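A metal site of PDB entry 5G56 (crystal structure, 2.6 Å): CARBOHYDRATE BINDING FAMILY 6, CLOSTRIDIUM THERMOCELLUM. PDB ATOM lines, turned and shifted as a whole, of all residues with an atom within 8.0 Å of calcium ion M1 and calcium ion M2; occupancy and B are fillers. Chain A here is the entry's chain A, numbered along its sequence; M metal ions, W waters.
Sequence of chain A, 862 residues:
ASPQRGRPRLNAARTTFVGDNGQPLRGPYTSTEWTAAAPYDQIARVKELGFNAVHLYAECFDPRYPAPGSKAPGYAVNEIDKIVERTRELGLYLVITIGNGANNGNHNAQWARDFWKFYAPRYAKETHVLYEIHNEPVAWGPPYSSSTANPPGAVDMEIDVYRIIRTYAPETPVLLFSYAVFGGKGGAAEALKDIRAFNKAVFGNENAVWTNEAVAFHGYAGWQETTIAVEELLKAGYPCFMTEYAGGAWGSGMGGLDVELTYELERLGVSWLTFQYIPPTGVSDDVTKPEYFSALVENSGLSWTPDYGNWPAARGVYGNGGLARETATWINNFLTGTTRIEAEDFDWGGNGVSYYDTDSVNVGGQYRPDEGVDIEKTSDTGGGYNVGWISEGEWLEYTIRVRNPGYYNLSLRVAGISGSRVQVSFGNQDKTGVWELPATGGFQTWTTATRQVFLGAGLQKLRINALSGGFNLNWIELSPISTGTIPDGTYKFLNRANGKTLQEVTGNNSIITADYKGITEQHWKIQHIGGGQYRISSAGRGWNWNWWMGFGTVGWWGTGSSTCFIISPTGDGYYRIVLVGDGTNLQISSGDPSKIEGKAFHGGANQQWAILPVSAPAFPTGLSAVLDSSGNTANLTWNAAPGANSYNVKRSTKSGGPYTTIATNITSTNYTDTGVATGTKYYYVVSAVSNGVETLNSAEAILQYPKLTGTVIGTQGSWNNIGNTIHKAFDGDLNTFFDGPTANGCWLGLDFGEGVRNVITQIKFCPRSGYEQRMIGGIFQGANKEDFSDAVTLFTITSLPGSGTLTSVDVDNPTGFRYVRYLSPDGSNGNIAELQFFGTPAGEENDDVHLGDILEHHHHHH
The backbone NH of Val 363 lies close to the side-chain carboxylate of Asp 374, 2.8 Å away. O of Asp 374 lies within hydrogen-bond range of N of Gly 388 (2.8 Å). The backbone NH of Ser 391 lies close to the side-chain carboxylate of Glu 394 (3.2 Å). N of Asp 357 sits at hydrogen-bond distance from OD1 of Asn 351 (2.9 Å). The side-chain carboxylate of Glu 394 is in hydrogen-bond range of the backbone NH of Thr 358, 2.8 Å away. The backbone NH (N) of Gly 372 is in hydrogen-bond range of the side-chain hydroxyl (OH) of Tyr 355 (2.9 Å).
The nearest printed residue that does not touch calcium ion M1 is Asn 362 (4.5 Å).
Within 4 Å of calcium ion M2: Asp 357, Asp 374, Trp 389 and Glu 394. The nearest printed residue that does not touch calcium ion M2 is Gly 388 (4.1 Å).
Calcium ion M1 is bound by the side-chain carboxylate (OD1) of Asp 359 (2.2 Å). OD2 of Asp 357 is bound to calcium ion M1, at 2.4 Å. Calcium ion M1 is bound by the backbone carbonyl oxygen (O) of Val 361 (2.4 Å). Calcium ion M1 is bound by O of Gly 372 (2.5 Å). Calcium ion M1 is bound by the side-chain carboxylate (OD2) of Asp 374 (2.6 Å). Calcium ion M1 is bound by OD1 of Asp 374 (2.7 Å).
Calcium ion M2 is bound by water W2, the side-chain carboxylate (OD1) of Asp 357, the backbone carbonyl oxygen (O) of Trp 389, water W1, the side-chain carboxylate (OD2) of Asp 374 and the side-chain carboxylate (OE1) of Glu 394. Slightly farther from calcium ion M2 lies the side-chain carboxylate (OE2) of Glu 394 (2.9 Å). Slightly farther from calcium ion M2 lies OD2 of Asp 357 (3.0 Å).
Water W1 lies within hydrogen-bond range of OG1 of Thr 358 (2.8 Å) and OE2 of Glu 394 (2.9 Å). Water W2 lies within hydrogen-bond range of O of Gly 388 (2.8 Å) and N of Asp 374 (3.3 Å).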
ATOM      1  N   ASN A 351      11.913  28.573  -0.282  1.00  0.00           N
ATOM      2  CA  ASN A 351      11.621  27.305   0.368  1.00  0.00           C
ATOM      3  C   ASN A 351      10.210  27.416   0.888  1.00  0.00           C
ATOM      4  O   ASN A 351       9.881  28.377   1.584  1.00  0.00           O
ATOM      5  CB  ASN A 351      12.607  27.020   1.511  1.00  0.00           C
ATOM      6  CG  ASN A 351      12.878  25.538   1.697  1.00  0.00           C
ATOM      7  OD1 ASN A 351      12.073  24.700   1.311  1.00  0.00           O
ATOM      8  ND2 ASN A 351      14.025  25.207   2.293  1.00  0.00           N
ATOM      9  N   TYR A 355       9.757  25.499  -4.248  1.00  0.00           N
ATOM     10  CA  TYR A 355      10.273  24.169  -3.915  1.00  0.00           C
ATOM     11  C   TYR A 355      10.138  23.988  -2.405  1.00  0.00           C
ATOM     12  O   TYR A 355       9.953  24.980  -1.686  1.00  0.00           O
ATOM     13  CB  TYR A 355      11.751  23.993  -4.330  1.00  0.00           C
ATOM     14  CG  TYR A 355      12.712  24.918  -3.594  1.00  0.00           C
ATOM     15  CD1 TYR A 355      12.993  26.192  -4.078  1.00  0.00           C
ATOM     16  CD2 TYR A 355      13.330  24.507  -2.413  1.00  0.00           C
ATOM     17  CE1 TYR A 355      13.857  27.041  -3.411  1.00  0.00           C
ATOM     18  CE2 TYR A 355      14.187  25.361  -1.732  1.00  0.00           C
ATOM     19  CZ  TYR A 355      14.447  26.617  -2.228  1.00  0.00           C
ATOM     20  OH  TYR A 355      15.312  27.466  -1.561  1.00  0.00           O
ATOM     21  N   TYR A 356      10.197  22.749  -1.940  1.00  0.00           N
ATOM     22  CA  TYR A 356      10.425  22.479  -0.518  1.00  0.00           C
ATOM     23  C   TYR A 356      11.614  21.534  -0.407  1.00  0.00           C
ATOM     24  O   TYR A 356      11.658  20.474  -1.043  1.00  0.00           O
ATOM     25  CB  TYR A 356       9.163  21.910   0.181  1.00  0.00           C
ATOM     26  CG  TYR A 356       9.478  21.331   1.556  1.00  0.00           C
ATOM     27  CD1 TYR A 356       9.875  22.158   2.619  1.00  0.00           C
ATOM     28  CD2 TYR A 356       9.428  19.948   1.780  1.00  0.00           C
ATOM     29  CE1 TYR A 356      10.195  21.611   3.874  1.00  0.00           C
ATOM     30  CE2 TYR A 356       9.744  19.398   3.013  1.00  0.00           C
ATOM     31  CZ  TYR A 356      10.128  20.220   4.056  1.00  0.00           C
ATOM     32  OH  TYR A 356      10.435  19.650   5.284  1.00  0.00           O
ATOM     33  N   ASP A 357      12.601  21.952   0.390  1.00  0.00           N
ATOM     34  CA  ASP A 357      13.742  21.128   0.757  1.00  0.00           C
ATOM     35  C   ASP A 357      13.885  21.136   2.280  1.00  0.00           C
ATOM     36  O   ASP A 357      13.567  22.130   2.943  1.00  0.00           O
ATOM     37  CB  ASP A 357      15.018  21.666   0.119  1.00  0.00           C
ATOM     38  CG  ASP A 357      16.094  20.608  -0.009  1.00  0.00           C
ATOM     39  OD1 ASP A 357      16.050  19.815  -0.967  1.00  0.00           O
ATOM     40  OD2 ASP A 357      16.994  20.535   0.846  1.00  0.00           O
ATOM     41  N   THR A 358      14.385  20.035   2.835  1.00  0.00           N
ATOM     42  CA  THR A 358      14.437  19.838   4.298  1.00  0.00           C
ATOM     43  C   THR A 358      15.400  20.769   5.046  1.00  0.00           C
ATOM     44  O   THR A 358      15.288  20.905   6.259  1.00  0.00           O
ATOM     45  CB  THR A 358      14.729  18.377   4.669  1.00  0.00           C
ATOM     46  OG1 THR A 358      15.891  17.924   3.971  1.00  0.00           O
ATOM     47  CG2 THR A 358      13.554  17.496   4.296  1.00  0.00           C
ATOM     48  N   ASP A 359      16.346  21.400   4.340  1.00  0.00           N
ATOM     49  CA  ASP A 359      17.182  22.466   4.925  1.00  0.00           C
ATOM     50  C   ASP A 359      17.426  23.589   3.923  1.00  0.00           C
ATOM     51  O   ASP A 359      17.124  23.446   2.735  1.00  0.00           O
ATOM     52  CB  ASP A 359      18.504  21.916   5.506  1.00  0.00           C
ATOM     53  CG  ASP A 359      19.392  21.232   4.456  1.00  0.00           C
ATOM     54  OD1 ASP A 359      19.488  21.727   3.319  1.00  0.00           O
ATOM     55  OD2 ASP A 359      20.024  20.201   4.768  1.00  0.00           O
ATOM     56  N   SER A 360      17.955  24.694   4.416  1.00  0.00           N
ATOM     57  CA  SER A 360      18.175  25.896   3.608  1.00  0.00           C
ATOM     58  C   SER A 360      19.541  25.974   2.904  1.00  0.00           C
ATOM     59  O   SER A 360      19.816  26.951   2.203  1.00  0.00           O
ATOM     60  CB  SER A 360      17.976  27.122   4.506  1.00  0.00           C
ATOM     61  OG  SER A 360      18.892  27.088   5.587  1.00  0.00           O
ATOM     62  N   VAL A 361      20.403  24.967   3.088  1.00  0.00           N
ATOM     63  CA  VAL A 361      21.703  24.939   2.405  1.00  0.00           C
ATOM     64  C   VAL A 361      21.660  24.001   1.194  1.00  0.00           C
ATOM     65  O   VAL A 361      20.922  23.001   1.192  1.00  0.00           O
ATOM     66  CB  VAL A 361      22.896  24.575   3.346  1.00  0.00           C
ATOM     67  CG1 VAL A 361      22.794  25.333   4.658  1.00  0.00           C
ATOM     68  CG2 VAL A 361      22.987  23.082   3.600  1.00  0.00           C
ATOM     69  N   ASN A 362      22.449  24.339   0.176  1.00  0.00           N
ATOM     70  CA  ASN A 362      22.718  23.466  -0.964  1.00  0.00           C
ATOM     71  C   ASN A 362      23.970  22.657  -0.594  1.00  0.00           C
ATOM     72  O   ASN A 362      25.089  23.119  -0.792  1.00  0.00           O
ATOM     73  CB  ASN A 362      22.936  24.316  -2.223  1.00  0.00           C
ATOM     74  CG  ASN A 362      23.262  23.501  -3.463  1.00  0.00           C
ATOM     75  OD1 ASN A 362      23.195  22.279  -3.461  1.00  0.00           O
ATOM     76  ND2 ASN A 362      23.626  24.186  -4.530  1.00  0.00           N
ATOM     77  N   VAL A 363      23.763  21.461  -0.046  1.00  0.00           N
ATOM     78  CA  VAL A 363      24.874  20.628   0.433  1.00  0.00           C
ATOM     79  C   VAL A 363      25.759  20.111  -0.701  1.00  0.00           C
ATOM     80  O   VAL A 363      26.935  19.809  -0.489  1.00  0.00           O
ATOM     81  CB  VAL A 363      24.424  19.419   1.320  1.00  0.00           C
ATOM     82  CG1 VAL A 363      23.584  19.889   2.503  1.00  0.00           C
ATOM     83  CG2 VAL A 363      23.698  18.355   0.497  1.00  0.00           C
ATOM     84  N   GLY A 364      25.186  19.990  -1.898  1.00  0.00           N
ATOM     85  CA  GLY A 364      25.941  19.625  -3.091  1.00  0.00           C
ATOM     86  C   GLY A 364      26.900  20.704  -3.564  1.00  0.00           C
ATOM     87  O   GLY A 364      28.017  20.398  -4.019  1.00  0.00           O
ATOM     88  N   GLU A 371      20.281  28.840  -2.685  1.00  0.00           N
ATOM     89  CA  GLU A 371      18.983  28.190  -2.521  1.00  0.00           C
ATOM     90  C   GLU A 371      19.086  26.840  -1.824  1.00  0.00           C
ATOM     91  O   GLU A 371      20.159  26.224  -1.760  1.00  0.00           O
ATOM     92  CB  GLU A 371      18.312  28.029  -3.894  1.00  0.00           C
ATOM     93  CG  GLU A 371      17.648  29.305  -4.397  1.00  0.00           C
ATOM     94  CD  GLU A 371      17.389  29.309  -5.880  1.00  0.00           C
ATOM     95  OE1 GLU A 371      18.351  29.507  -6.649  1.00  0.00           O
ATOM     96  OE2 GLU A 371      16.212  29.125  -6.276  1.00  0.00           O
ATOM     97  N   GLY A 372      17.955  26.371  -1.302  1.00  0.00           N
ATOM     98  CA  GLY A 372      17.900  25.149  -0.505  1.00  0.00           C
ATOM     99  C   GLY A 372      18.000  23.813  -1.224  1.00  0.00           C
ATOM    100  O   GLY A 372      18.293  22.806  -0.571  1.00  0.00           O
ATOM    101  N   VAL A 373      17.767  23.769  -2.535  1.00  0.00           N
ATOM    102  CA  VAL A 373      17.780  22.499  -3.299  1.00  0.00           C
ATOM    103  C   VAL A 373      19.222  21.993  -3.440  1.00  0.00           C
ATOM    104  O   VAL A 373      20.158  22.791  -3.593  1.00  0.00           O
ATOM    105  CB  VAL A 373      17.106  22.628  -4.681  1.00  0.00           C
ATOM    106  CG1 VAL A 373      17.133  21.308  -5.454  1.00  0.00           C
ATOM    107  CG2 VAL A 373      15.666  23.121  -4.534  1.00  0.00           C
ATOM    108  N   ASP A 374      19.389  20.671  -3.393  1.00  0.00           N
ATOM    109  CA  ASP A 374      20.704  20.059  -3.338  1.00  0.00           C
ATOM    110  C   ASP A 374      21.169  19.538  -4.704  1.00  0.00           C
ATOM    111  O   ASP A 374      20.592  18.597  -5.249  1.00  0.00           O
ATOM    112  CB  ASP A 374      20.705  18.965  -2.262  1.00  0.00           C
ATOM    113  CG  ASP A 374      20.433  19.532  -0.880  1.00  0.00           C
ATOM    114  OD1 ASP A 374      21.175  20.429  -0.461  1.00  0.00           O
ATOM    115  OD2 ASP A 374      19.443  19.117  -0.221  1.00  0.00           O
ATOM    116  N   ILE A 375      22.210  20.173  -5.225  1.00  0.00           N
ATOM    117  CA  ILE A 375      22.626  20.032  -6.624  1.00  0.00           C
ATOM    118  C   ILE A 375      24.108  19.625  -6.709  1.00  0.00           C
ATOM    119  O   ILE A 375      24.955  20.228  -6.067  1.00  0.00           O
ATOM    120  CB  ILE A 375      22.393  21.368  -7.363  1.00  0.00           C
ATOM    121  CG1 ILE A 375      21.018  21.942  -7.041  1.00  0.00           C
ATOM    122  CG2 ILE A 375      22.537  21.191  -8.877  1.00  0.00           C
ATOM    123  CD1 ILE A 375      20.717  23.245  -7.722  1.00  0.00           C
ATOM    124  N   VAL A 387      19.862  17.141  -9.490  1.00  0.00           N
ATOM    125  CA  VAL A 387      19.324  17.301  -8.133  1.00  0.00           C
ATOM    126  C   VAL A 387      19.543  15.985  -7.396  1.00  0.00           C
ATOM    127  O   VAL A 387      19.115  14.932  -7.871  1.00  0.00           O
ATOM    128  CB  VAL A 387      17.804  17.638  -8.129  1.00  0.00           C
ATOM    129  CG1 VAL A 387      17.227  17.605  -6.709  1.00  0.00           C
ATOM    130  CG2 VAL A 387      17.567  19.010  -8.757  1.00  0.00           C
ATOM    131  N   GLY A 388      20.252  16.052  -6.268  1.00  0.00           N
ATOM    132  CA  GLY A 388      20.433  14.908  -5.356  1.00  0.00           C
ATOM    133  C   GLY A 388      19.965  15.237  -3.958  1.00  0.00           C
ATOM    134  O   GLY A 388      19.400  16.300  -3.713  1.00  0.00           O
ATOM    135  N   TRP A 389      20.208  14.318  -3.016  1.00  0.00           N
ATOM    136  CA  TRP A 389      19.748  14.479  -1.622  1.00  0.00           C
ATOM    137  C   TRP A 389      18.217  14.709  -1.521  1.00  0.00           C
ATOM    138  O   TRP A 389      17.756  15.571  -0.774  1.00  0.00           O
ATOM    139  CB  TRP A 389      20.520  15.603  -0.906  1.00  0.00           C
ATOM    140  CG  TRP A 389      21.991  15.357  -0.783  1.00  0.00           C
ATOM    141  CD1 TRP A 389      22.635  14.788   0.274  1.00  0.00           C
ATOM    142  CD2 TRP A 389      23.017  15.695  -1.735  1.00  0.00           C
ATOM    143  NE1 TRP A 389      23.979  14.751   0.053  1.00  0.00           N
ATOM    144  CE2 TRP A 389      24.248  15.294  -1.170  1.00  0.00           C
ATOM    145  CE3 TRP A 389      23.017  16.302  -2.997  1.00  0.00           C
ATOM    146  CZ2 TRP A 389      25.467  15.470  -1.842  1.00  0.00           C
ATOM    147  CZ3 TRP A 389      24.237  16.475  -3.659  1.00  0.00           C
ATOM    148  CH2 TRP A 389      25.444  16.055  -3.073  1.00  0.00           C
ATOM    149  N   ILE A 390      17.458  13.933  -2.294  1.00  0.00           N
ATOM    150  CA  ILE A 390      16.003  14.069  -2.339  1.00  0.00           C
ATOM    151  C   ILE A 390      15.424  13.276  -1.175  1.00  0.00           C
ATOM    152  O   ILE A 390      15.444  12.047  -1.205  1.00  0.00           O
ATOM    153  CB  ILE A 390      15.424  13.577  -3.692  1.00  0.00           C
ATOM    154  CG1 ILE A 390      16.000  14.401  -4.856  1.00  0.00           C
ATOM    155  CG2 ILE A 390      13.898  13.666  -3.705  1.00  0.00           C
ATOM    156  CD1 ILE A 390      15.656  13.866  -6.232  1.00  0.00           C
ATOM    157  N   SER A 391      14.952  13.964  -0.140  1.00  0.00           N
ATOM    158  CA  SER A 391      14.222  13.350   0.978  1.00  0.00           C
ATOM    159  C   SER A 391      12.728  13.311   0.667  1.00  0.00           C
ATOM    160  O   SER A 391      12.249  14.141  -0.113  1.00  0.00           O
ATOM    161  CB  SER A 391      14.446  14.115   2.285  1.00  0.00           C
ATOM    162  OG  SER A 391      15.780  13.963   2.728  1.00  0.00           O
ATOM    163  N   GLU A 392      12.015  12.364   1.281  1.00  0.00           N
ATOM    164  CA  GLU A 392      10.569  12.248   1.074  1.00  0.00           C
ATOM    165  C   GLU A 392       9.863  13.466   1.649  1.00  0.00           C
ATOM    166  O   GLU A 392      10.318  14.033   2.645  1.00  0.00           O
ATOM    167  CB  GLU A 392       9.989  10.910   1.613  1.00  0.00           C
ATOM    168  CG  GLU A 392       9.600  10.836   3.085  1.00  0.00           C
ATOM    169  CD  GLU A 392       8.898   9.519   3.421  1.00  0.00           C
ATOM    170  OE1 GLU A 392       9.574   8.489   3.584  1.00  0.00           O
ATOM    171  OE2 GLU A 392       7.660   9.516   3.530  1.00  0.00           O
ATOM    172  N   GLU A 394       9.829  16.234  -0.042  1.00  0.00           N
ATOM    173  CA  GLU A 394      10.370  17.331  -0.837  1.00  0.00           C
ATOM    174  C   GLU A 394       9.666  17.449  -2.162  1.00  0.00           C
ATOM    175  O   GLU A 394       9.041  16.486  -2.651  1.00  0.00           O
ATOM    176  CB  GLU A 394      11.882  17.190  -1.043  1.00  0.00           C
ATOM    177  CG  GLU A 394      12.661  17.360   0.255  1.00  0.00           C
ATOM    178  CD  GLU A 394      14.150  17.507   0.042  1.00  0.00           C
ATOM    179  OE1 GLU A 394      14.659  17.023  -0.997  1.00  0.00           O
ATOM    180  OE2 GLU A 394      14.825  18.087   0.908  1.00  0.00           O
ATOM    181  N   TRP A 395       9.753  18.633  -2.753  1.00  0.00           N
ATOM    182  CA  TRP A 395       9.163  18.875  -4.051  1.00  0.00           C
ATOM    183  C   TRP A 395       9.800  20.048  -4.777  1.00  0.00           C
ATOM    184  O   TRP A 395      10.500  20.874  -4.189  1.00  0.00           O
ATOM    185  CB  TRP A 395       7.631  19.047  -3.937  1.00  0.00           C
ATOM    186  CG  TRP A 395       7.133  20.044  -2.911  1.00  0.00           C
ATOM    187  CD1 TRP A 395       6.733  19.777  -1.620  1.00  0.00           C
ATOM    188  CD2 TRP A 395       6.941  21.448  -3.108  1.00  0.00           C
ATOM    189  NE1 TRP A 395       6.328  20.932  -1.002  1.00  0.00           N
ATOM    190  CE2 TRP A 395       6.449  21.975  -1.885  1.00  0.00           C
ATOM    191  CE3 TRP A 395       7.148  22.320  -4.185  1.00  0.00           C
ATOM    192  CZ2 TRP A 395       6.154  23.333  -1.719  1.00  0.00           C
ATOM    193  CZ3 TRP A 395       6.855  23.675  -4.010  1.00  0.00           C
ATOM    194  CH2 TRP A 395       6.357  24.169  -2.786  1.00  0.00           C
ATOM    195  N   LEU A 396       9.570  20.058  -6.091  1.00  0.00           N
ATOM    196  CA  LEU A 396      10.176  21.002  -7.016  1.00  0.00           C
ATOM    197  C   LEU A 396       9.090  21.429  -8.003  1.00  0.00           C
ATOM    198  O   LEU A 396       8.446  20.565  -8.595  1.00  0.00           O
ATOM    199  CB  LEU A 396      11.336  20.326  -7.746  1.00  0.00           C
ATOM    200  CG  LEU A 396      12.477  19.745  -6.888  1.00  0.00           C
ATOM    201  CD1 LEU A 396      13.328  18.760  -7.653  1.00  0.00           C
ATOM    202  CD2 LEU A 396      13.354  20.855  -6.330  1.00  0.00           C
HETATM  203 CA    CA M   1      19.213  21.327   1.165  1.00  0.00          CA
HETATM  204 CA    CA M   2      17.359  17.914  -0.557  1.00  0.00          CA
HETATM  205  O   HOH W   1      17.605  17.756   1.825  1.00  0.00           O
HETATM  206  O   HOH W   2      17.399  18.034  -2.853  1.00  0.00           O
